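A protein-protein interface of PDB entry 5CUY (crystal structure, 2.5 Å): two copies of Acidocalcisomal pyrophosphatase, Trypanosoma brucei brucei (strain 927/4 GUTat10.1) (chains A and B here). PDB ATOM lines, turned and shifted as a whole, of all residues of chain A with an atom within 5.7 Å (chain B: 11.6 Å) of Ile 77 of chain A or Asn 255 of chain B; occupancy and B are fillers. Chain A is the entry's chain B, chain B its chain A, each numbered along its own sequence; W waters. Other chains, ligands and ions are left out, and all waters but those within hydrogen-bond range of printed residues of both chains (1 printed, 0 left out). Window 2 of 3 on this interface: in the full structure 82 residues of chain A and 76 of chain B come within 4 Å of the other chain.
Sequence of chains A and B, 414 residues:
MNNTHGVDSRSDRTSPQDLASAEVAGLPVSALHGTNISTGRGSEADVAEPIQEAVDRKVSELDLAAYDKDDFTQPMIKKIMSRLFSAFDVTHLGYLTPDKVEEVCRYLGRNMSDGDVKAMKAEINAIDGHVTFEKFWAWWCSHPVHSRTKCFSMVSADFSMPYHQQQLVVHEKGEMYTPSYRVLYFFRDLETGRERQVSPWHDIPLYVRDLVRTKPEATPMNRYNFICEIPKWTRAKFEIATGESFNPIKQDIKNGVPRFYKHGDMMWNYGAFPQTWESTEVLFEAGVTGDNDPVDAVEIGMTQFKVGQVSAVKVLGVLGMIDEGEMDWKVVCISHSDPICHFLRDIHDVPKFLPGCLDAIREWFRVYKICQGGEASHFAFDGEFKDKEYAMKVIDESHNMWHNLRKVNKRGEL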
ATOM      1  N   PHE A  72     -20.475  -2.804  24.256  1.00  0.00           N
ATOM      2  CA  PHE A  72     -21.352  -2.072  25.167  1.00  0.00           C
ATOM      3  C   PHE A  72     -21.809  -3.044  26.309  1.00  0.00           C
ATOM      4  O   PHE A  72     -22.035  -4.235  26.059  1.00  0.00           O
ATOM      5  CB  PHE A  72     -22.549  -1.552  24.370  1.00  0.00           C
ATOM      6  CG  PHE A  72     -22.283  -0.276  23.615  1.00  0.00           C
ATOM      7  CD1 PHE A  72     -20.998   0.159  23.371  1.00  0.00           C
ATOM      8  CD2 PHE A  72     -23.341   0.547  23.230  1.00  0.00           C
ATOM      9  CE1 PHE A  72     -20.770   1.401  22.771  1.00  0.00           C
ATOM     10  CE2 PHE A  72     -23.117   1.786  22.634  1.00  0.00           C
ATOM     11  CZ  PHE A  72     -21.828   2.215  22.410  1.00  0.00           C
ATOM     12  N   THR A  73     -21.928  -2.555  27.542  1.00  0.00           N
ATOM     13  CA  THR A  73     -22.372  -3.374  28.674  1.00  0.00           C
ATOM     14  C   THR A  73     -23.855  -3.659  28.511  1.00  0.00           C
ATOM     15  O   THR A  73     -24.537  -2.907  27.795  1.00  0.00           O
ATOM     16  CB  THR A  73     -22.201  -2.637  30.035  1.00  0.00           C
ATOM     17  OG1 THR A  73     -22.860  -1.362  29.983  1.00  0.00           O
ATOM     18  CG2 THR A  73     -20.741  -2.488  30.400  1.00  0.00           C
ATOM     19  N   GLN A  74     -24.400  -4.681  29.182  1.00  0.00           N
ATOM     20  CA  GLN A  74     -25.845  -4.936  28.986  1.00  0.00           C
ATOM     21  C   GLN A  74     -26.727  -3.676  29.252  1.00  0.00           C
ATOM     22  O   GLN A  74     -27.699  -3.422  28.534  1.00  0.00           O
ATOM     23  CB  GLN A  74     -26.340  -6.141  29.813  1.00  0.00           C
ATOM     24  CG  GLN A  74     -27.747  -6.590  29.371  1.00  0.00           C
ATOM     25  CD  GLN A  74     -28.297  -7.915  30.029  1.00  0.00           C
ATOM     26  OE1 GLN A  74     -28.451  -8.031  31.270  1.00  0.00           O
ATOM     27  NE2 GLN A  74     -28.624  -8.896  29.172  1.00  0.00           N
ATOM     28  N   PRO A  75     -26.393  -2.875  30.284  1.00  0.00           N
ATOM     29  CA  PRO A  75     -27.189  -1.673  30.560  1.00  0.00           C
ATOM     30  C   PRO A  75     -27.067  -0.677  29.414  1.00  0.00           C
ATOM     31  O   PRO A  75     -27.998   0.042  29.085  1.00  0.00           O
ATOM     32  CB  PRO A  75     -26.584  -1.151  31.848  1.00  0.00           C
ATOM     33  CG  PRO A  75     -26.177  -2.371  32.540  1.00  0.00           C
ATOM     34  CD  PRO A  75     -25.514  -3.179  31.433  1.00  0.00           C
ATOM     35  N   MET A  76     -25.926  -0.655  28.761  1.00  0.00           N
ATOM     36  CA  MET A  76     -25.785   0.258  27.642  1.00  0.00           C
ATOM     37  C   MET A  76     -26.608  -0.245  26.483  1.00  0.00           C
ATOM     38  O   MET A  76     -27.337   0.530  25.867  1.00  0.00           O
ATOM     39  CB  MET A  76     -24.329   0.387  27.214  1.00  0.00           C
ATOM     40  CG  MET A  76     -23.503   1.075  28.232  1.00  0.00           C
ATOM     41  SD  MET A  76     -21.732   0.774  28.010  1.00  0.00           S
ATOM     42  CE  MET A  76     -21.376   1.979  26.576  1.00  0.00           C
ATOM     43  N   ILE A  77     -26.520  -1.533  26.178  1.00  0.00           N
ATOM     44  CA  ILE A  77     -27.283  -2.015  25.037  1.00  0.00           C
ATOM     45  C   ILE A  77     -28.749  -1.756  25.228  1.00  0.00           C
ATOM     46  O   ILE A  77     -29.439  -1.333  24.305  1.00  0.00           O
ATOM     47  CB  ILE A  77     -27.060  -3.529  24.784  1.00  0.00           C
ATOM     48  CG1 ILE A  77     -25.664  -3.734  24.189  1.00  0.00           C
ATOM     49  CG2 ILE A  77     -28.112  -4.075  23.804  1.00  0.00           C
ATOM     50  CD1 ILE A  77     -25.059  -5.159  24.448  1.00  0.00           C
ATOM     51  N   LYS A  78     -29.225  -2.006  26.440  1.00  0.00           N
ATOM     52  CA  LYS A  78     -30.638  -1.828  26.721  1.00  0.00           C
ATOM     53  C   LYS A  78     -31.065  -0.360  26.471  1.00  0.00           C
ATOM     54  O   LYS A  78     -32.056  -0.120  25.782  1.00  0.00           O
ATOM     55  CB  LYS A  78     -30.939  -2.274  28.158  1.00  0.00           C
ATOM     56  CG  LYS A  78     -32.400  -2.472  28.451  1.00  0.00           C
ATOM     57  CD  LYS A  78     -32.641  -2.854  29.925  1.00  0.00           C
ATOM     58  CE  LYS A  78     -34.149  -2.960  30.240  1.00  0.00           C
ATOM     59  NZ  LYS A  78     -34.497  -3.533  31.596  1.00  0.00           N
ATOM     60  N   LYS A  79     -30.327   0.598  27.037  1.00  0.00           N
ATOM     61  CA  LYS A  79     -30.628   2.012  26.846  1.00  0.00           C
ATOM     62  C   LYS A  79     -30.678   2.327  25.346  1.00  0.00           C
ATOM     63  O   LYS A  79     -31.597   3.020  24.878  1.00  0.00           O
ATOM     64  CB  LYS A  79     -29.571   2.886  27.567  1.00  0.00           C
ATOM     65  CG  LYS A  79     -29.873   3.143  29.074  1.00  0.00           C
ATOM     66  CD  LYS A  79     -28.655   2.912  30.085  1.00  0.00           C
ATOM     67  CE  LYS A  79     -27.512   3.934  30.043  1.00  0.00           C
ATOM     68  NZ  LYS A  79     -27.790   5.275  30.715  1.00  0.00           N
ATOM     69  N   ILE A  80     -29.729   1.802  24.580  1.00  0.00           N
ATOM     70  CA  ILE A  80     -29.720   2.036  23.134  1.00  0.00           C
ATOM     71  C   ILE A  80     -30.886   1.370  22.404  1.00  0.00           C
ATOM     72  O   ILE A  80     -31.500   1.982  21.510  1.00  0.00           O
ATOM     73  CB  ILE A  80     -28.410   1.525  22.466  1.00  0.00           C
ATOM     74  CG1 ILE A  80     -27.221   2.325  22.986  1.00  0.00           C
ATOM     75  CG2 ILE A  80     -28.504   1.604  20.945  1.00  0.00           C
ATOM     76  CD1 ILE A  80     -27.276   3.810  22.617  1.00  0.00           C
ATOM     77  N   MET A  81     -31.199   0.121  22.760  1.00  0.00           N
ATOM     78  CA  MET A  81     -32.293  -0.571  22.081  1.00  0.00           C
ATOM     79  C   MET A  81     -33.626   0.094  22.330  1.00  0.00           C
ATOM     80  O   MET A  81     -34.534   0.059  21.514  1.00  0.00           O
ATOM     81  CB  MET A  81     -32.331  -2.034  22.492  1.00  0.00           C
ATOM     82  CG  MET A  81     -31.568  -2.844  21.518  1.00  0.00           C
ATOM     83  SD  MET A  81     -31.461  -4.521  21.989  1.00  0.00           S
ATOM     84  CE  MET A  81     -32.986  -5.205  21.304  1.00  0.00           C
ATOM     85  N   SER A  82     -33.730   0.715  23.483  1.00  0.00           N
ATOM     86  CA  SER A  82     -34.913   1.435  23.870  1.00  0.00           C
ATOM     87  C   SER A  82     -34.999   2.780  23.061  1.00  0.00           C
ATOM     88  O   SER A  82     -36.079   3.260  22.744  1.00  0.00           O
ATOM     89  CB  SER A  82     -34.825   1.634  25.369  1.00  0.00           C
ATOM     90  OG  SER A  82     -35.829   2.483  25.839  1.00  0.00           O
ATOM     91  N   LEU A 108     -32.834  -3.802  14.416  1.00  0.00           N
ATOM     92  CA  LEU A 108     -31.797  -3.975  15.452  1.00  0.00           C
ATOM     93  C   LEU A 108     -30.759  -5.030  15.042  1.00  0.00           C
ATOM     94  O   LEU A 108     -29.797  -5.291  15.770  1.00  0.00           O
ATOM     95  CB  LEU A 108     -32.419  -4.357  16.797  1.00  0.00           C
ATOM     96  CG  LEU A 108     -33.576  -3.458  17.214  1.00  0.00           C
ATOM     97  CD1 LEU A 108     -33.992  -3.747  18.637  1.00  0.00           C
ATOM     98  CD2 LEU A 108     -33.159  -2.015  17.044  1.00  0.00           C
ATOM     99  N   GLY A 109     -30.957  -5.642  13.878  1.00  0.00           N
ATOM    100  CA  GLY A 109     -29.996  -6.613  13.384  1.00  0.00           C
ATOM    101  C   GLY A 109     -30.271  -8.076  13.661  1.00  0.00           C
ATOM    102  O   GLY A 109     -29.347  -8.873  13.802  1.00  0.00           O
ATOM    103  N   TRP A 137     -37.812  -6.386  25.293  1.00  0.00           N
ATOM    104  CA  TRP A 137     -36.477  -6.603  25.792  1.00  0.00           C
ATOM    105  C   TRP A 137     -36.356  -7.939  26.538  1.00  0.00           C
ATOM    106  O   TRP A 137     -35.398  -8.698  26.320  1.00  0.00           O
ATOM    107  CB  TRP A 137     -36.056  -5.394  26.666  1.00  0.00           C
ATOM    108  CG  TRP A 137     -34.786  -5.596  27.475  1.00  0.00           C
ATOM    109  CD1 TRP A 137     -34.701  -5.758  28.819  1.00  0.00           C
ATOM    110  CD2 TRP A 137     -33.452  -5.607  26.992  1.00  0.00           C
ATOM    111  NE1 TRP A 137     -33.407  -5.859  29.206  1.00  0.00           N
ATOM    112  CE2 TRP A 137     -32.612  -5.768  28.101  1.00  0.00           C
ATOM    113  CE3 TRP A 137     -32.882  -5.497  25.725  1.00  0.00           C
ATOM    114  CZ2 TRP A 137     -31.218  -5.814  27.990  1.00  0.00           C
ATOM    115  CZ3 TRP A 137     -31.494  -5.545  25.597  1.00  0.00           C
ATOM    116  CH2 TRP A 137     -30.677  -5.698  26.724  1.00  0.00           C
ATOM    117  N   TRP A 140     -36.233 -10.408  23.958  1.00  0.00           N
ATOM    118  CA  TRP A 140     -34.953 -10.312  23.288  1.00  0.00           C
ATOM    119  C   TRP A 140     -33.822 -11.065  24.007  1.00  0.00           C
ATOM    120  O   TRP A 140     -33.066 -11.775  23.356  1.00  0.00           O
ATOM    121  CB  TRP A 140     -34.563  -8.840  23.107  1.00  0.00           C
ATOM    122  CG  TRP A 140     -33.337  -8.657  22.225  1.00  0.00           C
ATOM    123  CD1 TRP A 140     -32.016  -8.747  22.605  1.00  0.00           C
ATOM    124  CD2 TRP A 140     -33.326  -8.401  20.810  1.00  0.00           C
ATOM    125  NE1 TRP A 140     -31.203  -8.563  21.513  1.00  0.00           N
ATOM    126  CE2 TRP A 140     -31.981  -8.348  20.404  1.00  0.00           C
ATOM    127  CE3 TRP A 140     -34.320  -8.211  19.857  1.00  0.00           C
ATOM    128  CZ2 TRP A 140     -31.615  -8.110  19.091  1.00  0.00           C
ATOM    129  CZ3 TRP A 140     -33.949  -7.969  18.547  1.00  0.00           C
ATOM    130  CH2 TRP A 140     -32.619  -7.918  18.176  1.00  0.00           C
ATOM    131  N   TYR B 177     -24.151   4.822   9.684  1.00  0.00           N
ATOM    132  CA  TYR B 177     -23.900   4.357  11.059  1.00  0.00           C
ATOM    133  C   TYR B 177     -25.188   4.115  11.808  1.00  0.00           C
ATOM    134  O   TYR B 177     -25.244   4.187  13.008  1.00  0.00           O
ATOM    135  CB  TYR B 177     -22.986   5.305  11.831  1.00  0.00           C
ATOM    136  CG  TYR B 177     -21.712   5.609  11.086  1.00  0.00           C
ATOM    137  CD1 TYR B 177     -20.768   4.610  10.820  1.00  0.00           C
ATOM    138  CD2 TYR B 177     -21.448   6.903  10.619  1.00  0.00           C
ATOM    139  CE1 TYR B 177     -19.588   4.907  10.109  1.00  0.00           C
ATOM    140  CE2 TYR B 177     -20.278   7.197   9.905  1.00  0.00           C
ATOM    141  CZ  TYR B 177     -19.357   6.203   9.659  1.00  0.00           C
ATOM    142  OH  TYR B 177     -18.196   6.534   8.986  1.00  0.00           O
ATOM    143  N   THR B 178     -26.252   3.847  11.074  1.00  0.00           N
ATOM    144  CA  THR B 178     -27.517   3.509  11.707  1.00  0.00           C
ATOM    145  C   THR B 178     -28.059   2.355  10.865  1.00  0.00           C
ATOM    146  O   THR B 178     -27.608   2.147   9.759  1.00  0.00           O
ATOM    147  CB  THR B 178     -28.505   4.691  11.744  1.00  0.00           C
ATOM    148  OG1 THR B 178     -29.132   4.824  10.472  1.00  0.00           O
ATOM    149  CG2 THR B 178     -27.775   5.993  12.141  1.00  0.00           C
ATOM    150  N   PRO B 179     -28.994   1.565  11.402  1.00  0.00           N
ATOM    151  CA  PRO B 179     -29.569   0.429  10.659  1.00  0.00           C
ATOM    152  C   PRO B 179     -30.270   0.796   9.341  1.00  0.00           C
ATOM    153  O   PRO B 179     -30.544  -0.091   8.527  1.00  0.00           O
ATOM    154  CB  PRO B 179     -30.557  -0.179  11.654  1.00  0.00           C
ATOM    155  CG  PRO B 179     -29.944   0.207  13.005  1.00  0.00           C
ATOM    156  CD  PRO B 179     -29.518   1.628  12.778  1.00  0.00           C
ATOM    157  N   LYS B 250     -25.230  -2.551   3.282  1.00  0.00           N
ATOM    158  CA  LYS B 250     -25.750  -2.204   4.627  1.00  0.00           C
ATOM    159  C   LYS B 250     -24.652  -2.424   5.668  1.00  0.00           C
ATOM    160  O   LYS B 250     -23.634  -3.088   5.400  1.00  0.00           O
ATOM    161  CB  LYS B 250     -26.964  -3.047   5.022  1.00  0.00           C
ATOM    162  CG  LYS B 250     -26.656  -4.453   5.501  1.00  0.00           C
ATOM    163  CD  LYS B 250     -27.953  -5.155   5.936  1.00  0.00           C
ATOM    164  CE  LYS B 250     -27.718  -6.441   6.779  1.00  0.00           C
ATOM    165  NZ  LYS B 250     -29.015  -7.131   7.159  1.00  0.00           N
ATOM    166  N   GLN B 251     -24.837  -1.867   6.863  1.00  0.00           N
ATOM    167  CA  GLN B 251     -23.826  -2.048   7.904  1.00  0.00           C
ATOM    168  C   GLN B 251     -24.251  -3.151   8.824  1.00  0.00           C
ATOM    169  O   GLN B 251     -25.436  -3.398   8.994  1.00  0.00           O
ATOM    170  CB  GLN B 251     -23.620  -0.786   8.747  1.00  0.00           C
ATOM    171  CG  GLN B 251     -22.331  -0.875   9.599  1.00  0.00           C
ATOM    172  CD  GLN B 251     -22.010   0.400  10.385  1.00  0.00           C
ATOM    173  OE1 GLN B 251     -22.585   1.489  10.144  1.00  0.00           O
ATOM    174  NE2 GLN B 251     -21.073   0.275  11.324  1.00  0.00           N
ATOM    175  N   ASP B 252     -23.267  -3.812   9.407  1.00  0.00           N
ATOM    176  CA  ASP B 252     -23.520  -4.872  10.349  1.00  0.00           C
ATOM    177  C   ASP B 252     -23.988  -4.194  11.673  1.00  0.00           C
ATOM    178  O   ASP B 252     -23.351  -3.264  12.188  1.00  0.00           O
ATOM    179  CB  ASP B 252     -22.217  -5.690  10.526  1.00  0.00           C
ATOM    180  CG  ASP B 252     -22.395  -6.973  11.388  1.00  0.00           C
ATOM    181  OD1 ASP B 252     -23.535  -7.402  11.628  1.00  0.00           O
ATOM    182  OD2 ASP B 252     -21.382  -7.568  11.812  1.00  0.00           O
ATOM    183  N   ILE B 253     -25.135  -4.631  12.179  1.00  0.00           N
ATOM    184  CA  ILE B 253     -25.665  -4.112  13.433  1.00  0.00           C
ATOM    185  C   ILE B 253     -25.916  -5.256  14.448  1.00  0.00           C
ATOM    186  O   ILE B 253     -26.437  -6.323  14.086  1.00  0.00           O
ATOM    187  CB  ILE B 253     -26.994  -3.391  13.199  1.00  0.00           C
ATOM    188  CG1 ILE B 253     -26.875  -2.431  12.009  1.00  0.00           C
ATOM    189  CG2 ILE B 253     -27.422  -2.714  14.486  1.00  0.00           C
ATOM    190  CD1 ILE B 253     -25.897  -1.228  12.234  1.00  0.00           C
ATOM    191  N   LYS B 254     -25.567  -5.046  15.714  1.00  0.00           N
ATOM    192  CA  LYS B 254     -25.786  -6.070  16.734  1.00  0.00           C
ATOM    193  C   LYS B 254     -26.326  -5.421  17.981  1.00  0.00           C
ATOM    194  O   LYS B 254     -25.623  -4.676  18.698  1.00  0.00           O
ATOM    195  CB  LYS B 254     -24.496  -6.826  17.077  1.00  0.00           C
ATOM    196  CG  LYS B 254     -24.694  -8.100  17.902  1.00  0.00           C
ATOM    197  CD  LYS B 254     -23.357  -8.822  18.124  1.00  0.00           C
ATOM    198  CE  LYS B 254     -23.473 -10.135  18.983  1.00  0.00           C
ATOM    199  NZ  LYS B 254     -24.440 -11.192  18.442  1.00  0.00           N
ATOM    200  N   ASN B 255     -27.593  -5.731  18.229  1.00  0.00           N
ATOM    201  CA  ASN B 255     -28.325  -5.228  19.365  1.00  0.00           C
ATOM    202  C   ASN B 255     -28.440  -3.734  19.208  1.00  0.00           C
ATOM    203  O   ASN B 255     -28.218  -3.009  20.162  1.00  0.00           O
ATOM    204  CB  ASN B 255     -27.584  -5.571  20.652  1.00  0.00           C
ATOM    205  CG  ASN B 255     -27.415  -7.066  20.833  1.00  0.00           C
ATOM    206  OD1 ASN B 255     -28.366  -7.839  20.650  1.00  0.00           O
ATOM    207  ND2 ASN B 255     -26.206  -7.487  21.201  1.00  0.00           N
ATOM    208  N   GLY B 256     -28.763  -3.273  18.006  1.00  0.00           N
ATOM    209  CA  GLY B 256     -28.901  -1.849  17.774  1.00  0.00           C
ATOM    210  C   GLY B 256     -27.615  -1.007  17.725  1.00  0.00           C
ATOM    211  O   GLY B 256     -27.660   0.221  17.500  1.00  0.00           O
ATOM    212  N   VAL B 257     -26.465  -1.637  17.932  1.00  0.00           N
ATOM    213  CA  VAL B 257     -25.244  -0.873  17.896  1.00  0.00           C
ATOM    214  C   VAL B 257     -24.485  -1.211  16.630  1.00  0.00           C
ATOM    215  O   VAL B 257     -24.362  -2.383  16.270  1.00  0.00           O
ATOM    216  CB  VAL B 257     -24.343  -1.198  19.080  1.00  0.00           C
ATOM    217  CG1 VAL B 257     -23.223  -0.188  19.142  1.00  0.00           C
ATOM    218  CG2 VAL B 257     -25.150  -1.232  20.383  1.00  0.00           C
ATOM    219  N   PRO B 258     -23.960  -0.185  15.936  1.00  0.00           N
ATOM    220  CA  PRO B 258     -23.187  -0.317  14.689  1.00  0.00           C
ATOM    221  C   PRO B 258     -21.876  -1.103  14.953  1.00  0.00           C
ATOM    222  O   PRO B 258     -21.130  -0.769  15.883  1.00  0.00           O
ATOM    223  CB  PRO B 258     -22.891   1.141  14.315  1.00  0.00           C
ATOM    224  CG  PRO B 258     -23.914   1.930  15.061  1.00  0.00           C
ATOM    225  CD  PRO B 258     -24.017   1.219  16.360  1.00  0.00           C
ATOM    226  N   ARG B 259     -21.602  -2.128  14.148  1.00  0.00           N
ATOM    227  CA  ARG B 259     -20.402  -2.948  14.309  1.00  0.00           C
ATOM    228  C   ARG B 259     -19.175  -2.395  13.566  1.00  0.00           C
ATOM    229  O   ARG B 259     -19.267  -1.868  12.445  1.00  0.00           O
ATOM    230  CB  ARG B 259     -20.655  -4.380  13.805  1.00  0.00           C
ATOM    231  CG  ARG B 259     -21.476  -5.328  14.675  1.00  0.00           C
ATOM    232  CD  ARG B 259     -20.584  -6.096  15.622  1.00  0.00           C
ATOM    233  NE  ARG B 259     -20.920  -7.529  15.696  1.00  0.00           N
ATOM    234  CZ  ARG B 259     -20.541  -8.467  14.821  1.00  0.00           C
ATOM    235  NH1 ARG B 259     -19.793  -8.156  13.765  1.00  0.00           N
ATOM    236  NH2 ARG B 259     -20.912  -9.734  15.009  1.00  0.00           N
ATOM    237  N   PHE B 260     -18.018  -2.569  14.199  1.00  0.00           N
ATOM    238  CA  PHE B 260     -16.719  -2.134  13.683  1.00  0.00           C
ATOM    239  C   PHE B 260     -15.689  -3.231  13.902  1.00  0.00           C
ATOM    240  O   PHE B 260     -15.880  -4.137  14.707  1.00  0.00           O
ATOM    241  CB  PHE B 260     -16.259  -0.873  14.433  1.00  0.00           C
ATOM    242  CG  PHE B 260     -17.150   0.310  14.220  1.00  0.00           C
ATOM    243  CD1 PHE B 260     -16.933   1.177  13.126  1.00  0.00           C
ATOM    244  CD2 PHE B 260     -18.245   0.521  15.048  1.00  0.00           C
ATOM    245  CE1 PHE B 260     -17.792   2.214  12.866  1.00  0.00           C
ATOM    246  CE2 PHE B 260     -19.124   1.569  14.796  1.00  0.00           C
ATOM    247  CZ  PHE B 260     -18.896   2.418  13.696  1.00  0.00           C
ATOM    248  N   LYS B 262     -12.567  -4.368  15.612  1.00  0.00           N
ATOM    249  CA  LYS B 262     -11.922  -3.817  16.782  1.00  0.00           C
ATOM    250  C   LYS B 262     -10.411  -3.977  16.699  1.00  0.00           C
ATOM    251  O   LYS B 262      -9.651  -3.261  17.370  1.00  0.00           O
ATOM    252  CB  LYS B 262     -12.499  -4.440  18.063  1.00  0.00           C
ATOM    253  CG  LYS B 262     -13.983  -3.979  18.412  1.00  0.00           C
ATOM    254  CD  LYS B 262     -14.114  -2.408  18.434  1.00  0.00           C
ATOM    255  CE  LYS B 262     -15.476  -1.838  18.869  1.00  0.00           C
ATOM    256  NZ  LYS B 262     -15.641  -1.674  20.370  1.00  0.00           N
HETATM  257  O   HOH W   1     -28.748  -8.089  16.851  1.00  0.00           O
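The backbone NH (N) of Asn 255 of chain B is in hydrogen-bond range of the backbone carbonyl oxygen (O) of Leu 108 of chain A (3.3 Å).
The indole nitrogen of Trp 140 of chain A is in hydrogen-bond range of the side-chain amide oxygen of Asn 255 of chain B (3.1 Å).
The backbone carbonyl oxygen (O) of Leu 108 of chain A sits at hydrogen-bond distance from the backbone NH (N) of Gly 256 of chain B (3.2 Å).
Among the printed residues, merely in contact across the chains: Phe 72 of chain A with Val 257 of chain B, Ile 77 of chain A with Asn 255 of chain B, Ile 80 of chain A with Gly 256 of chain B, Met 81 of chain A with Asn 255 of chain B, Leu 108 of chain A with Ile 253 of chain B and Gly 109 of chain A with Ile 253 of chain B.
No residue of chain B comes within 4 Å of Pro 75 of chain A.
No residue of chain B comes within 4 Å of Met 76 of chain A.
Lys 78 of chain A touches none of the printed residues of chain B.
Of the printed residues of chain B, Ile 80 of chain A touches Gly 256.
Met 81 of chain A touches one residue of chain B.
Leu 108 of chain A touches three residues of chain B.
Of the printed residues of chain B, Trp 140 of chain A touches Asn 255.
Of the printed residues of chain A, Ile 253 of chain B touches Leu 108 (3.7 Å) and Gly 109 (3.6 Å).
Of chain A, only Ile 77 (3.5 Å), Met 81 (3.6 Å), Leu 108 (3.3 Å) and Trp 140 (3.1 Å) come within 4 Å of Asn 255 of chain B.
Printed residues of chain A within 4 Å of Val 257 of chain B: Phe 72 (3.8 Å).
The nearest residue of chain B that does not touch Ile 77 of chain A is Val 257 of chain B (4.6 Å).
Printed residues of chain A that touch a printed residue of chain B: Phe 72, Ile 77, Ile 80, Met 81, Leu 108, Gly 109 and Trp 140.
Hydrophobic or aromatic side chains of chain A that line the printed part of chain B: Phe 72, Ile 77, Ile 80, Met 81 and Trp 140.
Among the printed residues, 9 pairs touch across the chains.
Among the printed residues, no Asp or Glu carboxylate lies within 4 Å of a Lys or Arg side-chain nitrogen of the other chain.
No position is printed for both chains.
Water W1 lies within hydrogen-bond range of the backbone NH of Asn 255 of chain B, the backbone carbonyl oxygen of Leu 108 of chain A and the backbone carbonyl oxygen of Gly 109 of chain A.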
